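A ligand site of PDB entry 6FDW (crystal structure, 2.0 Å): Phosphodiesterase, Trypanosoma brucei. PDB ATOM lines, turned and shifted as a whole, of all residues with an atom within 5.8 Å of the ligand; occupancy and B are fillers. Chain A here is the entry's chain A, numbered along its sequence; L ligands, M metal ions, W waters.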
ATOM      1  N   TYR A 110      16.516 -21.800  -1.165  1.00  0.00           N
ATOM      2  CA  TYR A 110      15.432 -21.282  -0.256  1.00  0.00           C
ATOM      3  C   TYR A 110      15.890 -20.064   0.563  1.00  0.00           C
ATOM      4  O   TYR A 110      15.318 -19.007   0.438  1.00  0.00           O
ATOM      5  CB  TYR A 110      14.910 -22.379   0.685  1.00  0.00           C
ATOM      6  CG  TYR A 110      13.750 -21.924   1.551  1.00  0.00           C
ATOM      7  CD1 TYR A 110      12.448 -21.802   1.013  1.00  0.00           C
ATOM      8  CD2 TYR A 110      13.945 -21.506   2.830  1.00  0.00           C
ATOM      9  CE1 TYR A 110      11.381 -21.326   1.771  1.00  0.00           C
ATOM     10  CE2 TYR A 110      12.872 -21.036   3.618  1.00  0.00           C
ATOM     11  CZ  TYR A 110      11.570 -20.965   3.088  1.00  0.00           C
ATOM     12  OH  TYR A 110      10.509 -20.515   3.848  1.00  0.00           O
ATOM     13  N   HIS A 111      16.908 -20.253   1.400  1.00  0.00           N
ATOM     14  CA  HIS A 111      17.404 -19.205   2.274  1.00  0.00           C
ATOM     15  C   HIS A 111      18.253 -18.164   1.636  1.00  0.00           C
ATOM     16  O   HIS A 111      19.345 -17.935   2.006  1.00  0.00           O
ATOM     17  CB  HIS A 111      18.140 -19.784   3.449  1.00  0.00           C
ATOM     18  CG  HIS A 111      17.262 -20.517   4.383  1.00  0.00           C
ATOM     19  ND1 HIS A 111      17.228 -21.876   4.444  1.00  0.00           N
ATOM     20  CD2 HIS A 111      16.372 -20.080   5.288  1.00  0.00           C
ATOM     21  CE1 HIS A 111      16.366 -22.244   5.362  1.00  0.00           C
ATOM     22  NE2 HIS A 111      15.828 -21.180   5.889  1.00  0.00           N
ATOM     23  N   THR A 225      14.121 -17.595  16.152  1.00  0.00           N
ATOM     24  CA  THR A 225      13.828 -18.336  14.928  1.00  0.00           C
ATOM     25  C   THR A 225      14.430 -19.711  14.824  1.00  0.00           C
ATOM     26  O   THR A 225      14.103 -20.472  13.886  1.00  0.00           O
ATOM     27  CB  THR A 225      14.205 -17.585  13.666  1.00  0.00           C
ATOM     28  OG1 THR A 225      15.646 -17.430  13.558  1.00  0.00           O
ATOM     29  CG2 THR A 225      13.504 -16.225  13.627  1.00  0.00           C
ATOM     30  N   MET A 227      14.343 -23.285  15.147  1.00  0.00           N
ATOM     31  CA  MET A 227      13.190 -24.216  15.293  1.00  0.00           C
ATOM     32  C   MET A 227      13.319 -25.248  16.430  1.00  0.00           C
ATOM     33  O   MET A 227      12.304 -25.853  16.825  1.00  0.00           O
ATOM     34  CB  MET A 227      12.782 -24.879  13.956  1.00  0.00           C
ATOM     35  CG  MET A 227      12.083 -23.945  12.900  1.00  0.00           C
ATOM     36  SD  MET A 227      10.559 -23.127  13.495  1.00  0.00           S
ATOM     37  CE  MET A 227       9.467 -24.558  13.542  1.00  0.00           C
ATOM     38  N   ASP A 264       8.333 -16.552   9.347  1.00  0.00           N
ATOM     39  CA  ASP A 264       9.272 -17.594   8.952  1.00  0.00           C
ATOM     40  C   ASP A 264       8.604 -18.873   8.506  1.00  0.00           C
ATOM     41  O   ASP A 264       9.125 -19.540   7.644  1.00  0.00           O
ATOM     42  CB  ASP A 264      10.181 -17.955  10.118  1.00  0.00           C
ATOM     43  CG  ASP A 264      11.653 -18.077   9.728  1.00  0.00           C
ATOM     44  OD1 ASP A 264      11.981 -17.889   8.555  1.00  0.00           O
ATOM     45  OD2 ASP A 264      12.446 -18.458  10.583  1.00  0.00           O
ATOM     46  N   ILE A 265       7.475 -19.236   9.138  1.00  0.00           N
ATOM     47  CA  ILE A 265       6.738 -20.461   8.750  1.00  0.00           C
ATOM     48  C   ILE A 265       5.397 -20.126   8.034  1.00  0.00           C
ATOM     49  O   ILE A 265       4.461 -20.938   8.041  1.00  0.00           O
ATOM     50  CB  ILE A 265       6.500 -21.424   9.959  1.00  0.00           C
ATOM     51  CG1 ILE A 265       5.709 -20.780  11.074  1.00  0.00           C
ATOM     52  CG2 ILE A 265       7.826 -22.026  10.504  1.00  0.00           C
ATOM     53  CD1 ILE A 265       5.375 -21.793  12.163  1.00  0.00           C
ATOM     54  N   ASN A 267       4.905 -19.840   4.687  1.00  0.00           N
ATOM     55  CA  ASN A 267       4.739 -20.280   3.287  1.00  0.00           C
ATOM     56  C   ASN A 267       3.357 -21.020   3.065  1.00  0.00           C
ATOM     57  O   ASN A 267       2.694 -20.822   2.052  1.00  0.00           O
ATOM     58  CB  ASN A 267       5.851 -21.198   2.877  1.00  0.00           C
ATOM     59  CG  ASN A 267       7.240 -20.516   2.807  1.00  0.00           C
ATOM     60  OD1 ASN A 267       8.206 -21.260   2.850  1.00  0.00           O
ATOM     61  ND2 ASN A 267       7.333 -19.196   2.728  1.00  0.00           N
ATOM     62  N   VAL A 268       2.938 -21.782   4.044  1.00  0.00           N
ATOM     63  CA  VAL A 268       1.682 -22.521   4.000  1.00  0.00           C
ATOM     64  C   VAL A 268       0.420 -21.683   4.191  1.00  0.00           C
ATOM     65  O   VAL A 268      -0.643 -22.207   4.148  1.00  0.00           O
ATOM     66  CB  VAL A 268       1.636 -23.685   5.005  1.00  0.00           C
ATOM     67  CG1 VAL A 268       2.629 -24.736   4.649  1.00  0.00           C
ATOM     68  CG2 VAL A 268       1.856 -23.198   6.390  1.00  0.00           C
ATOM     69  N   SER A 275       2.504 -21.307  -2.267  1.00  0.00           N
ATOM     70  CA  SER A 275       2.917 -22.196  -1.233  1.00  0.00           C
ATOM     71  C   SER A 275       3.680 -23.360  -1.828  1.00  0.00           C
ATOM     72  O   SER A 275       4.649 -23.799  -1.257  1.00  0.00           O
ATOM     73  CB  SER A 275       1.683 -22.669  -0.493  1.00  0.00           C
ATOM     74  OG  SER A 275       1.969 -23.444   0.617  1.00  0.00           O
ATOM     75  N   TRP A 278       7.245 -22.336  -2.821  1.00  0.00           N
ATOM     76  CA  TRP A 278       8.124 -22.305  -1.671  1.00  0.00           C
ATOM     77  C   TRP A 278       8.532 -23.709  -1.279  1.00  0.00           C
ATOM     78  O   TRP A 278       9.728 -23.974  -0.952  1.00  0.00           O
ATOM     79  CB  TRP A 278       7.473 -21.582  -0.455  1.00  0.00           C
ATOM     80  CG  TRP A 278       7.350 -20.123  -0.593  1.00  0.00           C
ATOM     81  CD1 TRP A 278       6.213 -19.446  -0.515  1.00  0.00           C
ATOM     82  CD2 TRP A 278       8.406 -19.150  -0.775  1.00  0.00           C
ATOM     83  NE1 TRP A 278       6.445 -18.113  -0.644  1.00  0.00           N
ATOM     84  CE2 TRP A 278       7.794 -17.901  -0.808  1.00  0.00           C
ATOM     85  CE3 TRP A 278       9.790 -19.219  -0.904  1.00  0.00           C
ATOM     86  CZ2 TRP A 278       8.507 -16.713  -0.999  1.00  0.00           C
ATOM     87  CZ3 TRP A 278      10.519 -18.004  -1.062  1.00  0.00           C
ATOM     88  CH2 TRP A 278       9.883 -16.787  -1.064  1.00  0.00           C
ATOM     89  N   ALA A 279       7.582 -24.628  -1.321  1.00  0.00           N
ATOM     90  CA  ALA A 279       7.850 -25.999  -0.944  1.00  0.00           C
ATOM     91  C   ALA A 279       8.881 -26.629  -1.854  1.00  0.00           C
ATOM     92  O   ALA A 279       9.701 -27.383  -1.412  1.00  0.00           O
ATOM     93  CB  ALA A 279       6.581 -26.802  -0.919  1.00  0.00           C
ATOM     94  N   VAL A 282      12.444 -25.195  -0.813  1.00  0.00           N
ATOM     95  CA  VAL A 282      12.992 -25.701   0.450  1.00  0.00           C
ATOM     96  C   VAL A 282      13.408 -27.189   0.344  1.00  0.00           C
ATOM     97  O   VAL A 282      14.427 -27.617   0.908  1.00  0.00           O
ATOM     98  CB  VAL A 282      12.082 -25.411   1.674  1.00  0.00           C
ATOM     99  CG1 VAL A 282      10.899 -26.346   1.737  1.00  0.00           C
ATOM    100  CG2 VAL A 282      12.876 -25.514   2.965  1.00  0.00           C
ATOM    101  N   PHE A 286      17.052 -28.694   1.121  1.00  0.00           N
ATOM    102  CA  PHE A 286      17.262 -29.856   1.954  1.00  0.00           C
ATOM    103  C   PHE A 286      18.046 -30.993   1.247  1.00  0.00           C
ATOM    104  O   PHE A 286      18.917 -31.646   1.868  1.00  0.00           O
ATOM    105  CB  PHE A 286      15.927 -30.380   2.447  1.00  0.00           C
ATOM    106  CG  PHE A 286      15.272 -29.506   3.511  1.00  0.00           C
ATOM    107  CD1 PHE A 286      15.911 -28.392   4.101  1.00  0.00           C
ATOM    108  CD2 PHE A 286      13.981 -29.829   3.936  1.00  0.00           C
ATOM    109  CE1 PHE A 286      15.278 -27.622   5.047  1.00  0.00           C
ATOM    110  CE2 PHE A 286      13.368 -29.088   4.935  1.00  0.00           C
ATOM    111  CZ  PHE A 286      14.021 -27.980   5.488  1.00  0.00           C
ATOM    112  N   MET A 303      14.166 -36.904   5.260  1.00  0.00           N
ATOM    113  CA  MET A 303      13.731 -35.637   4.722  1.00  0.00           C
ATOM    114  C   MET A 303      14.778 -34.966   3.840  1.00  0.00           C
ATOM    115  O   MET A 303      14.451 -34.163   2.992  1.00  0.00           O
ATOM    116  CB  MET A 303      13.392 -34.733   5.886  1.00  0.00           C
ATOM    117  CG  MET A 303      12.814 -33.402   5.492  1.00  0.00           C
ATOM    118  SD  MET A 303      12.514 -32.527   7.024  1.00  0.00           S
ATOM    119  CE  MET A 303      10.871 -31.899   6.766  1.00  0.00           C
ATOM    120  N   GLY A 315       4.885 -34.339   2.593  1.00  0.00           N
ATOM    121  CA  GLY A 315       5.806 -33.495   3.349  1.00  0.00           C
ATOM    122  C   GLY A 315       5.143 -32.175   3.746  1.00  0.00           C
ATOM    123  O   GLY A 315       5.246 -31.754   4.920  1.00  0.00           O
ATOM    124  N   GLN A 316       4.374 -31.582   2.825  1.00  0.00           N
ATOM    125  CA  GLN A 316       3.571 -30.410   3.185  1.00  0.00           C
ATOM    126  C   GLN A 316       2.458 -30.711   4.202  1.00  0.00           C
ATOM    127  O   GLN A 316       2.278 -30.008   5.177  1.00  0.00           O
ATOM    128  CB  GLN A 316       3.087 -29.678   1.958  1.00  0.00           C
ATOM    129  CG  GLN A 316       4.237 -29.021   1.196  1.00  0.00           C
ATOM    130  CD  GLN A 316       4.942 -27.933   1.967  1.00  0.00           C
ATOM    131  OE1 GLN A 316       4.322 -26.927   2.277  1.00  0.00           O
ATOM    132  NE2 GLN A 316       6.213 -28.139   2.280  1.00  0.00           N
ATOM    133  N   GLY A 318       2.446 -33.071   6.521  1.00  0.00           N
ATOM    134  CA  GLY A 318       3.083 -33.318   7.789  1.00  0.00           C
ATOM    135  C   GLY A 318       3.527 -32.018   8.458  1.00  0.00           C
ATOM    136  O   GLY A 318       3.306 -31.846   9.663  1.00  0.00           O
ATOM    137  N   PHE A 319       4.111 -31.115   7.674  1.00  0.00           N
ATOM    138  CA  PHE A 319       4.512 -29.789   8.198  1.00  0.00           C
ATOM    139  C   PHE A 319       3.312 -28.993   8.690  1.00  0.00           C
ATOM    140  O   PHE A 319       3.337 -28.393   9.744  1.00  0.00           O
ATOM    141  CB  PHE A 319       5.266 -29.003   7.135  1.00  0.00           C
ATOM    142  CG  PHE A 319       5.909 -27.740   7.635  1.00  0.00           C
ATOM    143  CD1 PHE A 319       6.967 -27.794   8.535  1.00  0.00           C
ATOM    144  CD2 PHE A 319       5.468 -26.491   7.194  1.00  0.00           C
ATOM    145  CE1 PHE A 319       7.553 -26.634   8.976  1.00  0.00           C
ATOM    146  CE2 PHE A 319       6.084 -25.327   7.606  1.00  0.00           C
ATOM    147  CZ  PHE A 319       7.115 -25.401   8.502  1.00  0.00           C
ATOM    148  N   PHE A 322       1.855 -31.083  11.999  1.00  0.00           N
ATOM    149  CA  PHE A 322       2.716 -31.098  13.172  1.00  0.00           C
ATOM    150  C   PHE A 322       3.266 -29.731  13.583  1.00  0.00           C
ATOM    151  O   PHE A 322       3.541 -29.534  14.755  1.00  0.00           O
ATOM    152  CB  PHE A 322       3.827 -32.126  13.014  1.00  0.00           C
ATOM    153  CG  PHE A 322       3.321 -33.549  13.006  1.00  0.00           C
ATOM    154  CD1 PHE A 322       2.811 -34.116  14.187  1.00  0.00           C
ATOM    155  CD2 PHE A 322       3.299 -34.308  11.821  1.00  0.00           C
ATOM    156  CE1 PHE A 322       2.292 -35.417  14.191  1.00  0.00           C
ATOM    157  CE2 PHE A 322       2.781 -35.609  11.825  1.00  0.00           C
ATOM    158  CZ  PHE A 322       2.287 -36.164  13.015  1.00  0.00           C
ATOM    159  N   VAL A 323       3.405 -28.788  12.660  1.00  0.00           N
ATOM    160  CA  VAL A 323       4.049 -27.520  13.002  1.00  0.00           C
ATOM    161  C   VAL A 323       3.104 -26.369  12.779  1.00  0.00           C
ATOM    162  O   VAL A 323       2.741 -25.705  13.746  1.00  0.00           O
ATOM    163  CB  VAL A 323       5.388 -27.321  12.268  1.00  0.00           C
ATOM    164  CG1 VAL A 323       5.978 -25.952  12.542  1.00  0.00           C
ATOM    165  CG2 VAL A 323       6.444 -28.368  12.634  1.00  0.00           C
HETATM  166  C1  LIG L   1       7.565 -24.681   2.362  1.00  0.00           C
HETATM  167  N1  LIG L   1      12.532 -26.374   9.175  1.00  0.00           N
HETATM  168  C2  LIG L   1       9.254 -24.312   4.599  1.00  0.00           C
HETATM  169  C3  LIG L   1      10.182 -24.213   5.609  1.00  0.00           C
HETATM  170  C4  LIG L   1      10.524 -25.314   6.368  1.00  0.00           C
HETATM  171  C5  LIG L   1      11.526 -25.252   7.471  1.00  0.00           C
HETATM  172  C6  LIG L   1       7.742 -31.903  10.577  1.00  0.00           C
HETATM  173  C7  LIG L   1       8.153 -31.955   8.167  1.00  0.00           C
HETATM  174  C8  LIG L   1       9.034 -31.149   8.787  1.00  0.00           C
HETATM  175  C9  LIG L   1       8.855 -31.174  10.218  1.00  0.00           C
HETATM  176  C10 LIG L   1      10.923 -28.527  11.802  1.00  0.00           C
HETATM  177  C11 LIG L   1      11.156 -27.344  10.930  1.00  0.00           C
HETATM  178  C12 LIG L   1      13.378 -25.367   9.506  1.00  0.00           C
HETATM  179  C13 LIG L   1      14.331 -23.033   8.919  1.00  0.00           C
HETATM  180  C14 LIG L   1      13.440 -22.064   9.628  1.00  0.00           C
HETATM  181  C15 LIG L   1      12.122 -22.071   9.561  1.00  0.00           C
HETATM  182  C16 LIG L   1      11.344 -23.061   8.758  1.00  0.00           C
HETATM  183  C17 LIG L   1       8.957 -26.669   5.075  1.00  0.00           C
HETATM  184  O1  LIG L   1       7.669 -25.719   3.350  1.00  0.00           O
HETATM  185  C18 LIG L   1       8.614 -25.524   4.330  1.00  0.00           C
HETATM  186  N2  LIG L   1      11.719 -26.349   8.107  1.00  0.00           N
HETATM  187  C19 LIG L   1      12.343 -27.593  10.011  1.00  0.00           C
HETATM  188  C20 LIG L   1      12.150 -28.876   9.203  1.00  0.00           C
HETATM  189  C21 LIG L   1      11.778 -30.061  10.059  1.00  0.00           C
HETATM  190  N3  LIG L   1      10.685 -29.739  10.997  1.00  0.00           N
HETATM  191  C22 LIG L   1       9.577 -30.539  11.242  1.00  0.00           C
HETATM  192  N4  LIG L   1       9.153 -30.712  12.524  1.00  0.00           N
HETATM  193  C23 LIG L   1       8.049 -31.460  12.785  1.00  0.00           C
HETATM  194  N5  LIG L   1       7.654 -31.619  14.083  1.00  0.00           N
HETATM  195  N6  LIG L   1       7.315 -32.078  11.835  1.00  0.00           N
HETATM  196  S1  LIG L   1       6.962 -32.611   9.235  1.00  0.00           S
HETATM  197  O2  LIG L   1      13.889 -25.339  10.622  1.00  0.00           O
HETATM  198  C24 LIG L   1      13.591 -24.299   8.448  1.00  0.00           C
HETATM  199  C25 LIG L   1      12.214 -23.931   7.829  1.00  0.00           C
HETATM  200  C26 LIG L   1       9.911 -26.542   6.101  1.00  0.00           C
HETATM  201  O3  LIG L   1       8.310 -27.823   4.716  1.00  0.00           O
HETATM  202  C27 LIG L   1       8.742 -29.076   5.253  1.00  0.00           C
HETATM  203 MG    MG M   1      16.764 -18.994  10.131  1.00  0.00          MG
HETATM  204 ZN    ZN M   2      14.104 -17.605   7.714  1.00  0.00          ZN
HETATM  205  O   HOH W   1      13.941 -19.762   7.358  1.00  0.00           O
HETATM  206  O   HOH W   2       4.606 -23.903   1.471  1.00  0.00           O
HETATM  207  O   HOH W   3      16.837 -25.080   7.398  1.00  0.00           O
HETATM  208  O   HOH W   4      16.658 -20.689   8.723  1.00  0.00           O
HETATM  209  O   HOH W   5      11.483 -20.634   6.632  1.00  0.00           O
HETATM  210  O   HOH W   6      15.532 -22.984  12.137  1.00  0.00           O
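Water W2 bridges the backbone carbonyl oxygen (O) of Ser 275 (2.7 Å) and the side-chain amide oxygen (OE1) of Gln 316 (3.1 Å).
Water W5 lies within hydrogen-bond range of the backbone carbonyl oxygen of Asp 264 and the side-chain hydroxyl of Tyr 110.
Water W6 lies within hydrogen-bond range of O2 of the ligand (3.2 Å), N of Met 227 (3.3 Å) and O of Thr 225 (3.4 Å).
The backbone carbonyl oxygen (O) of Gly 318 lies close to a sulfur (S1) of the ligand (3.8 Å).
Residues that only touch the ligand: Met 303, Met 227, Val 323, Asn 267, Val 282, Ala 279, Phe 322, Asp 264, Phe 286, His 111 and Trp 278.
Hydrophobic or aromatic side chains within 4 Å of the ligand: Met 227, Val 282, Phe 286, Met 303, Phe 319, Phe 322 and Val 323.
14 residues have an atom within 4 Å of the ligand: His 111, Met 227, Asp 264, Asn 267, Trp 278, Ala 279, Val 282, Phe 286, Met 303, Gln 316, Gly 318, Phe 319, Phe 322 and Val 323.
The side-chain hydroxyl of Tyr 110 sits at hydrogen-bond distance from the side-chain amide oxygen of Asn 267 (2.6 Å).
The backbone carbonyl oxygen (O) of Asn 267 sits at hydrogen-bond distance from the side-chain hydroxyl (OG) of Ser 275, at 3.1 Å.
O1 of the ligand lies within hydrogen-bond range of NE2 of Gln 316 (3.0 Å).
A sulfur (S1) of the ligand sits close to the backbone NH (N) of Phe 319 (3.6 Å).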
